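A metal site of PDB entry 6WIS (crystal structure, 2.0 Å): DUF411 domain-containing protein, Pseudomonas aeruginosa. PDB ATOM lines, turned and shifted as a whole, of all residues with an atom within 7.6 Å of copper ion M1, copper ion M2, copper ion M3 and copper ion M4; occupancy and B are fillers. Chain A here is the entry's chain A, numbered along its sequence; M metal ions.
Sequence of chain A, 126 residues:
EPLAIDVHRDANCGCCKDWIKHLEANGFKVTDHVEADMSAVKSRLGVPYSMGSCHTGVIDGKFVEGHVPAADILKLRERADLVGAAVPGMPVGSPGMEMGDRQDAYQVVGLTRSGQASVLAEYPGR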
ATOM      1  N   VAL A   7     -25.649  35.096 -32.576  1.00  0.00           N
ATOM      2  CA  VAL A   7     -25.606  33.752 -31.989  1.00  0.00           C
ATOM      3  C   VAL A   7     -25.796  32.704 -33.070  1.00  0.00           C
ATOM      4  O   VAL A   7     -26.788  32.728 -33.822  1.00  0.00           O
ATOM      5  CB  VAL A   7     -26.654  33.602 -30.880  1.00  0.00           C
ATOM      6  CG1 VAL A   7     -26.583  32.178 -30.274  1.00  0.00           C
ATOM      7  CG2 VAL A   7     -26.415  34.667 -29.790  1.00  0.00           C
ATOM      8  N   HIS A   8     -24.847  31.767 -33.150  1.00  0.00           N
ATOM      9  CA  HIS A   8     -24.968  30.558 -33.959  1.00  0.00           C
ATOM     10  C   HIS A   8     -25.309  29.421 -33.003  1.00  0.00           C
ATOM     11  O   HIS A   8     -24.531  29.146 -32.078  1.00  0.00           O
ATOM     12  CB  HIS A   8     -23.664  30.233 -34.707  1.00  0.00           C
ATOM     13  CG  HIS A   8     -22.960  31.431 -35.249  1.00  0.00           C
ATOM     14  ND1 HIS A   8     -22.891  31.713 -36.601  1.00  0.00           N
ATOM     15  CD2 HIS A   8     -22.272  32.420 -34.630  1.00  0.00           C
ATOM     16  CE1 HIS A   8     -22.209  32.817 -36.787  1.00  0.00           C
ATOM     17  NE2 HIS A   8     -21.819  33.271 -35.607  1.00  0.00           N
ATOM     18  N   ARG A   9     -26.464  28.784 -33.200  1.00  0.00           N
ATOM     19  CA  ARG A   9     -26.935  27.816 -32.199  1.00  0.00           C
ATOM     20  C   ARG A   9     -27.286  26.479 -32.823  1.00  0.00           C
ATOM     21  O   ARG A   9     -27.694  26.381 -33.981  1.00  0.00           O
ATOM     22  CB  ARG A   9     -28.140  28.376 -31.424  1.00  0.00           C
ATOM     23  CG  ARG A   9     -29.343  28.744 -32.280  1.00  0.00           C
ATOM     24  CD  ARG A   9     -30.543  29.142 -31.417  1.00  0.00           C
ATOM     25  NE  ARG A   9     -31.605  29.783 -32.184  1.00  0.00           N
ATOM     26  CZ  ARG A   9     -32.702  29.174 -32.630  1.00  0.00           C
ATOM     27  NH1 ARG A   9     -32.918  27.883 -32.402  1.00  0.00           N
ATOM     28  NH2 ARG A   9     -33.617  29.871 -33.301  1.00  0.00           N
ATOM     29  N   ASP A  10     -27.129  25.435 -32.008  1.00  0.00           N
ATOM     30  CA  ASP A  10     -27.485  24.064 -32.384  1.00  0.00           C
ATOM     31  C   ASP A  10     -28.948  23.971 -32.786  1.00  0.00           C
ATOM     32  O   ASP A  10     -29.816  24.648 -32.222  1.00  0.00           O
ATOM     33  CB  ASP A  10     -27.215  23.118 -31.224  1.00  0.00           C
ATOM     34  CG  ASP A  10     -25.786  22.663 -31.174  1.00  0.00           C
ATOM     35  OD1 ASP A  10     -24.999  23.044 -32.073  1.00  0.00           O
ATOM     36  OD2 ASP A  10     -25.434  21.904 -30.248  1.00  0.00           O
ATOM     37  N   ALA A  11     -29.227  23.143 -33.784  1.00  0.00           N
ATOM     38  CA  ALA A  11     -30.623  22.894 -34.140  1.00  0.00           C
ATOM     39  C   ALA A  11     -31.337  22.196 -33.001  1.00  0.00           C
ATOM     40  O   ALA A  11     -30.743  21.369 -32.286  1.00  0.00           O
ATOM     41  CB  ALA A  11     -30.714  22.050 -35.422  1.00  0.00           C
ATOM     42  N   ASN A  12     -32.620  22.539 -32.800  1.00  0.00           N
ATOM     43  CA  ASN A  12     -33.536  21.813 -31.898  1.00  0.00           C
ATOM     44  C   ASN A  12     -33.046  21.842 -30.447  1.00  0.00           C
ATOM     45  O   ASN A  12     -33.164  20.864 -29.718  1.00  0.00           O
ATOM     46  CB  ASN A  12     -33.752  20.363 -32.362  1.00  0.00           C
ATOM     47  CG  ASN A  12     -34.909  19.694 -31.606  1.00  0.00           C
ATOM     48  OD1 ASN A  12     -36.010  20.252 -31.527  1.00  0.00           O
ATOM     49  ND2 ASN A  12     -34.653  18.530 -31.013  1.00  0.00           N
ATOM     50  N   CYS A  13     -32.484  22.975 -30.031  1.00  0.00           N
ATOM     51  CA  CYS A  13     -31.895  23.123 -28.707  1.00  0.00           C
ATOM     52  C   CYS A  13     -32.661  24.239 -27.997  1.00  0.00           C
ATOM     53  O   CYS A  13     -32.562  25.411 -28.395  1.00  0.00           O
ATOM     54  CB  CYS A  13     -30.398  23.424 -28.810  1.00  0.00           C
ATOM     55  SG  CYS A  13     -29.466  23.254 -27.273  1.00  0.00           S
ATOM     56  N   GLY A  14     -33.439  23.875 -26.985  1.00  0.00           N
ATOM     57  CA  GLY A  14     -34.315  24.812 -26.310  1.00  0.00           C
ATOM     58  C   GLY A  14     -33.569  25.765 -25.391  1.00  0.00           C
ATOM     59  O   GLY A  14     -33.939  26.939 -25.306  1.00  0.00           O
ATOM     60  N   CYS A  15     -32.505  25.268 -24.744  1.00  0.00           N
ATOM     61  CA  CYS A  15     -31.735  26.097 -23.808  1.00  0.00           C
ATOM     62  C   CYS A  15     -31.066  27.282 -24.503  1.00  0.00           C
ATOM     63  O   CYS A  15     -30.974  28.368 -23.916  1.00  0.00           O
ATOM     64  CB  CYS A  15     -30.689  25.243 -23.086  1.00  0.00           C
ATOM     65  SG  CYS A  15     -29.799  24.210 -24.277  1.00  0.00           S
ATOM     66  N   CYS A  16     -30.586  27.100 -25.740  1.00  0.00           N
ATOM     67  CA  CYS A  16     -30.009  28.232 -26.484  1.00  0.00           C
ATOM     68  C   CYS A  16     -31.002  29.371 -26.625  1.00  0.00           C
ATOM     69  O   CYS A  16     -30.642  30.539 -26.460  1.00  0.00           O
ATOM     70  CB  CYS A  16     -29.538  27.802 -27.879  1.00  0.00           C
ATOM     71  SG  CYS A  16     -28.530  26.288 -28.012  1.00  0.00           S
ATOM     72  N   LYS A  17     -32.254  29.052 -26.959  1.00  0.00           N
ATOM     73  CA  LYS A  17     -33.284  30.073 -27.111  1.00  0.00           C
ATOM     74  C   LYS A  17     -33.621  30.738 -25.785  1.00  0.00           C
ATOM     75  O   LYS A  17     -33.917  31.941 -25.760  1.00  0.00           O
ATOM     76  CB  LYS A  17     -34.557  29.444 -27.719  1.00  0.00           C
ATOM     77  CG  LYS A  17     -34.403  28.993 -29.189  1.00  0.00           C
ATOM     78  CD  LYS A  17     -35.616  28.174 -29.673  1.00  0.00           C
ATOM     79  N   ASP A  18     -33.578  29.978 -24.690  1.00  0.00           N
ATOM     80  CA  ASP A  18     -33.803  30.549 -23.362  1.00  0.00           C
ATOM     81  C   ASP A  18     -32.659  31.485 -22.983  1.00  0.00           C
ATOM     82  O   ASP A  18     -32.885  32.580 -22.458  1.00  0.00           O
ATOM     83  CB  ASP A  18     -33.952  29.408 -22.340  1.00  0.00           C
ATOM     84  CG  ASP A  18     -34.403  29.886 -20.943  1.00  0.00           C
ATOM     85  OD1 ASP A  18     -34.970  30.974 -20.783  1.00  0.00           O
ATOM     86  OD2 ASP A  18     -34.206  29.146 -19.975  1.00  0.00           O
ATOM     87  N   TRP A  19     -31.408  31.076 -23.252  1.00  0.00           N
ATOM     88  CA  TRP A  19     -30.268  31.964 -23.007  1.00  0.00           C
ATOM     89  C   TRP A  19     -30.403  33.270 -23.797  1.00  0.00           C
ATOM     90  O   TRP A  19     -30.143  34.354 -23.254  1.00  0.00           O
ATOM     91  CB  TRP A  19     -28.984  31.229 -23.372  1.00  0.00           C
ATOM     92  CG  TRP A  19     -27.736  31.963 -23.186  1.00  0.00           C
ATOM     93  CD1 TRP A  19     -27.118  32.236 -22.000  1.00  0.00           C
ATOM     94  CD2 TRP A  19     -26.884  32.493 -24.211  1.00  0.00           C
ATOM     95  NE1 TRP A  19     -25.922  32.912 -22.230  1.00  0.00           N
ATOM     96  CE2 TRP A  19     -25.752  33.060 -23.587  1.00  0.00           C
ATOM     97  CE3 TRP A  19     -26.970  32.520 -25.615  1.00  0.00           C
ATOM     98  CZ2 TRP A  19     -24.714  33.652 -24.312  1.00  0.00           C
ATOM     99  CZ3 TRP A  19     -25.915  33.115 -26.341  1.00  0.00           C
ATOM    100  CH2 TRP A  19     -24.816  33.679 -25.691  1.00  0.00           C
ATOM    101  N   MET A  38     -21.240  23.977 -37.616  1.00  0.00           N
ATOM    102  CA  MET A  38     -20.826  24.459 -36.313  1.00  0.00           C
ATOM    103  C   MET A  38     -19.326  24.219 -36.064  1.00  0.00           C
ATOM    104  O   MET A  38     -18.675  25.038 -35.409  1.00  0.00           O
ATOM    105  CB  MET A  38     -21.663  23.812 -35.207  1.00  0.00           C
ATOM    106  CG  MET A  38     -21.317  24.364 -33.829  1.00  0.00           C
ATOM    107  SD  MET A  38     -21.872  26.259 -33.680  1.00  0.00           S
ATOM    108  CE  MET A  38     -23.680  25.935 -33.087  1.00  0.00           C
ATOM    109  N   SER A  53     -19.713  24.060 -26.654  1.00  0.00           N
ATOM    110  CA  SER A  53     -21.015  24.003 -25.997  1.00  0.00           C
ATOM    111  C   SER A  53     -22.031  23.901 -27.110  1.00  0.00           C
ATOM    112  O   SER A  53     -21.708  23.521 -28.245  1.00  0.00           O
ATOM    113  CB  SER A  53     -21.182  25.215 -25.065  1.00  0.00           C
ATOM    114  OG  SER A  53     -22.360  25.134 -24.280  1.00  0.00           O
ATOM    115  N   CYS A  54     -23.288  24.256 -26.808  1.00  0.00           N
ATOM    116  CA  CYS A  54     -24.414  24.100 -27.730  1.00  0.00           C
ATOM    117  C   CYS A  54     -24.649  25.315 -28.619  1.00  0.00           C
ATOM    118  O   CYS A  54     -25.470  25.254 -29.558  1.00  0.00           O
ATOM    119  CB  CYS A  54     -25.677  23.827 -26.903  1.00  0.00           C
ATOM    120  SG  CYS A  54     -25.786  25.019 -25.504  1.00  0.00           S
ATOM    121  N   HIS A  55     -23.995  26.447 -28.346  1.00  0.00           N
ATOM    122  CA  HIS A  55     -24.149  27.618 -29.194  1.00  0.00           C
ATOM    123  C   HIS A  55     -22.886  28.467 -29.095  1.00  0.00           C
ATOM    124  O   HIS A  55     -22.116  28.339 -28.141  1.00  0.00           O
ATOM    125  CB  HIS A  55     -25.384  28.447 -28.799  1.00  0.00           C
ATOM    126  CG  HIS A  55     -25.278  29.053 -27.422  1.00  0.00           C
ATOM    127  ND1 HIS A  55     -26.007  28.605 -26.342  1.00  0.00           N
ATOM    128  CD2 HIS A  55     -24.517  30.078 -26.960  1.00  0.00           C
ATOM    129  CE1 HIS A  55     -25.703  29.326 -25.268  1.00  0.00           C
ATOM    130  NE2 HIS A  55     -24.777  30.216 -25.615  1.00  0.00           N
ATOM    131  N   THR A  56     -22.693  29.356 -30.062  1.00  0.00           N
ATOM    132  CA  THR A  56     -21.524  30.235 -30.085  1.00  0.00           C
ATOM    133  C   THR A  56     -22.002  31.643 -30.430  1.00  0.00           C
ATOM    134  O   THR A  56     -22.603  31.848 -31.490  1.00  0.00           O
ATOM    135  CB  THR A  56     -20.476  29.785 -31.118  1.00  0.00           C
ATOM    136  OG1 THR A  56     -20.117  28.413 -30.874  1.00  0.00           O
ATOM    137  CG2 THR A  56     -19.225  30.670 -31.003  1.00  0.00           C
ATOM    138  N   GLU A  65     -18.940  31.266 -25.754  1.00  0.00           N
ATOM    139  CA  GLU A  65     -19.239  29.854 -25.985  1.00  0.00           C
ATOM    140  C   GLU A  65     -20.133  29.358 -24.857  1.00  0.00           C
ATOM    141  O   GLU A  65     -19.726  29.370 -23.686  1.00  0.00           O
ATOM    142  CB  GLU A  65     -17.954  29.034 -26.062  1.00  0.00           C
ATOM    143  CG  GLU A  65     -18.181  27.557 -26.389  1.00  0.00           C
ATOM    144  CD  GLU A  65     -18.681  27.339 -27.822  1.00  0.00           C
ATOM    145  OE1 GLU A  65     -18.618  28.315 -28.599  1.00  0.00           O
ATOM    146  OE2 GLU A  65     -19.134  26.208 -28.167  1.00  0.00           O
ATOM    147  N   GLY A  66     -21.340  28.955 -25.185  1.00  0.00           N
ATOM    148  CA  GLY A  66     -22.190  28.389 -24.159  1.00  0.00           C
ATOM    149  C   GLY A  66     -22.924  29.410 -23.284  1.00  0.00           C
ATOM    150  O   GLY A  66     -23.089  30.599 -23.603  1.00  0.00           O
ATOM    151  N   HIS A  67     -23.397  28.895 -22.156  1.00  0.00           N
ATOM    152  CA  HIS A  67     -24.340  29.619 -21.296  1.00  0.00           C
ATOM    153  C   HIS A  67     -23.609  30.594 -20.351  1.00  0.00           C
ATOM    154  O   HIS A  67     -23.691  30.503 -19.128  1.00  0.00           O
ATOM    155  CB  HIS A  67     -25.193  28.607 -20.554  1.00  0.00           C
ATOM    156  CG  HIS A  67     -26.151  27.885 -21.446  1.00  0.00           C
ATOM    157  ND1 HIS A  67     -27.445  28.323 -21.658  1.00  0.00           N
ATOM    158  CD2 HIS A  67     -26.002  26.803 -22.247  1.00  0.00           C
ATOM    159  CE1 HIS A  67     -28.044  27.536 -22.530  1.00  0.00           C
ATOM    160  NE2 HIS A  67     -27.188  26.606 -22.909  1.00  0.00           N
ATOM    161  N   GLY A  89     -19.813  22.691 -22.320  1.00  0.00           N
ATOM    162  CA  GLY A  89     -20.917  21.807 -21.993  1.00  0.00           C
ATOM    163  C   GLY A  89     -22.209  22.584 -21.741  1.00  0.00           C
ATOM    164  O   GLY A  89     -22.454  23.660 -22.302  1.00  0.00           O
ATOM    165  N   MET A  90     -23.056  22.011 -20.880  1.00  0.00           N
ATOM    166  CA  MET A  90     -24.303  22.673 -20.526  1.00  0.00           C
ATOM    167  C   MET A  90     -24.622  22.406 -19.074  1.00  0.00           C
ATOM    168  O   MET A  90     -25.465  21.561 -18.781  1.00  0.00           O
ATOM    169  CB  MET A  90     -25.458  22.182 -21.416  1.00  0.00           C
ATOM    170  CG  MET A  90     -25.290  22.368 -22.919  1.00  0.00           C
ATOM    171  SD  MET A  90     -26.831  21.693 -23.963  1.00  0.00           S
ATOM    172  CE  MET A  90     -26.812  19.818 -23.399  1.00  0.00           C
ATOM    173  N   PRO A  91     -23.951  23.123 -18.178  1.00  0.00           N
ATOM    174  CA  PRO A  91     -24.171  22.890 -16.733  1.00  0.00           C
ATOM    175  C   PRO A  91     -25.548  23.352 -16.320  1.00  0.00           C
ATOM    176  O   PRO A  91     -25.981  24.456 -16.669  1.00  0.00           O
ATOM    177  CB  PRO A  91     -23.074  23.718 -16.062  1.00  0.00           C
ATOM    178  CG  PRO A  91     -22.673  24.733 -17.098  1.00  0.00           C
ATOM    179  CD  PRO A  91     -22.863  24.087 -18.433  1.00  0.00           C
ATOM    180  N   SER A  94     -26.936  27.192 -15.092  1.00  0.00           N
ATOM    181  CA  SER A  94     -26.438  28.339 -15.827  1.00  0.00           C
ATOM    182  C   SER A  94     -27.592  29.009 -16.570  1.00  0.00           C
ATOM    183  O   SER A  94     -28.645  28.390 -16.773  1.00  0.00           O
ATOM    184  CB  SER A  94     -25.320  27.912 -16.791  1.00  0.00           C
ATOM    185  OG  SER A  94     -25.799  27.041 -17.811  1.00  0.00           O
ATOM    186  N   PRO A  95     -27.440  30.280 -16.959  1.00  0.00           N
ATOM    187  CA  PRO A  95     -28.584  31.001 -17.553  1.00  0.00           C
ATOM    188  C   PRO A  95     -29.040  30.365 -18.858  1.00  0.00           C
ATOM    189  O   PRO A  95     -28.245  30.109 -19.758  1.00  0.00           O
ATOM    190  CB  PRO A  95     -28.052  32.419 -17.778  1.00  0.00           C
ATOM    191  CG  PRO A  95     -26.782  32.528 -16.978  1.00  0.00           C
ATOM    192  CD  PRO A  95     -26.257  31.140 -16.769  1.00  0.00           C
ATOM    193  N   GLY A  96     -30.347  30.126 -18.954  1.00  0.00           N
ATOM    194  CA  GLY A  96     -30.903  29.387 -20.073  1.00  0.00           C
ATOM    195  C   GLY A  96     -30.900  27.893 -19.892  1.00  0.00           C
ATOM    196  O   GLY A  96     -31.568  27.192 -20.667  1.00  0.00           O
ATOM    197  N   MET A  97     -30.214  27.378 -18.882  1.00  0.00           N
ATOM    198  CA  MET A  97     -30.157  25.953 -18.536  1.00  0.00           C
ATOM    199  C   MET A  97     -30.702  25.755 -17.112  1.00  0.00           C
ATOM    200  O   MET A  97     -30.439  24.759 -16.468  1.00  0.00           O
ATOM    201  CB  MET A  97     -28.724  25.414 -18.626  1.00  0.00           C
ATOM    202  CG  MET A  97     -28.267  24.861 -20.054  1.00  0.00           C
ATOM    203  SD  MET A  97     -29.365  23.334 -20.673  1.00  0.00           S
ATOM    204  CE  MET A  97     -28.862  22.153 -19.168  1.00  0.00           C
ATOM    205  N   MET A  99     -32.944  24.787 -14.029  1.00  0.00           N
ATOM    206  CA  MET A  99     -34.014  23.818 -13.787  1.00  0.00           C
ATOM    207  C   MET A  99     -34.218  23.612 -12.272  1.00  0.00           C
ATOM    208  O   MET A  99     -33.889  22.549 -11.740  1.00  0.00           O
ATOM    209  CB  MET A  99     -33.679  22.478 -14.453  1.00  0.00           C
ATOM    210  CG  MET A  99     -33.506  22.570 -15.964  1.00  0.00           C
ATOM    211  SD  MET A  99     -33.085  20.928 -16.846  1.00  0.00           S
ATOM    212  CE  MET A  99     -32.787  21.697 -18.578  1.00  0.00           C
HETATM  213 CU    CU M   1     -27.733  25.133 -24.313  1.00  0.00          CU
HETATM  214 CU    CU M   2     -26.921  26.640 -26.599  1.00  0.00          CU
HETATM  215 CU    CU M   3     -29.654  25.298 -26.338  1.00  0.00          CU
HETATM  216 CU    CU M   4     -28.808  22.592 -22.893  1.00  0.00          CU
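Within 4 Å of copper ion M2: Cys 16, Cys 54, His 55 and His 67. The nearest printed residue that does not touch copper ion M2 is Cys 13 (4.3 Å).
Copper ion M4 is bound by SG of Cys 15 (2.3 Å), SD of Met 97 (2.4 Å) and SD of Met 90 (2.4 Å). Copper ion M4 has three donor atoms within binding distance.
Three residues have an atom within 4 Å of copper ion M4: Cys 15, Met 90 and Met 97. Along chain A the residues within 4 Å of copper ion M4 span positions 15 to 97. The nearest printed residue that does not touch copper ion M4 is His 67 (4.3 Å).
The side-chain sulfur (SG) of Cys 16 binds copper ion M2 (2.2 Å). ND1 of His 55 binds copper ion M2 (2.2 Å). SG of Cys 54 is bound to copper ion M2, 2.3 Å away. Copper ion M2 has three donor atoms within binding distance.
The side-chain hydroxyl of Ser 53 lies close to the side-chain sulfur of Cys 54 (3.6 Å). The backbone carbonyl oxygen (O) of Gly 66 sits at hydrogen-bond distance from a ring nitrogen (NE2) of His 55 (2.7 Å). O of Cys 54 lies within hydrogen-bond range of N of Asp 10, at 3.0 Å. A ring nitrogen (ND1) of His 67 is in hydrogen-bond range of the backbone carbonyl oxygen (O) of Pro 95, 2.7 Å away.
Within 4 Å of copper ion M3: Cys 13, Cys 15, Cys 16 and Cys 54. The nearest printed residue that does not touch copper ion M3 is Gly 14 (4.1 Å).
Copper ion M3 is bound by the backbone nitrogen of Cys 16 (2.1 Å), the side-chain sulfur of Cys 16 (2.2 Å), the side-chain sulfur of Cys 13 (2.3 Å) and the side-chain sulfur of Cys 15 (2.3 Å).
Copper ion M1 is bound by NE2 of His 67, SG of Cys 15 and SG of Cys 54.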
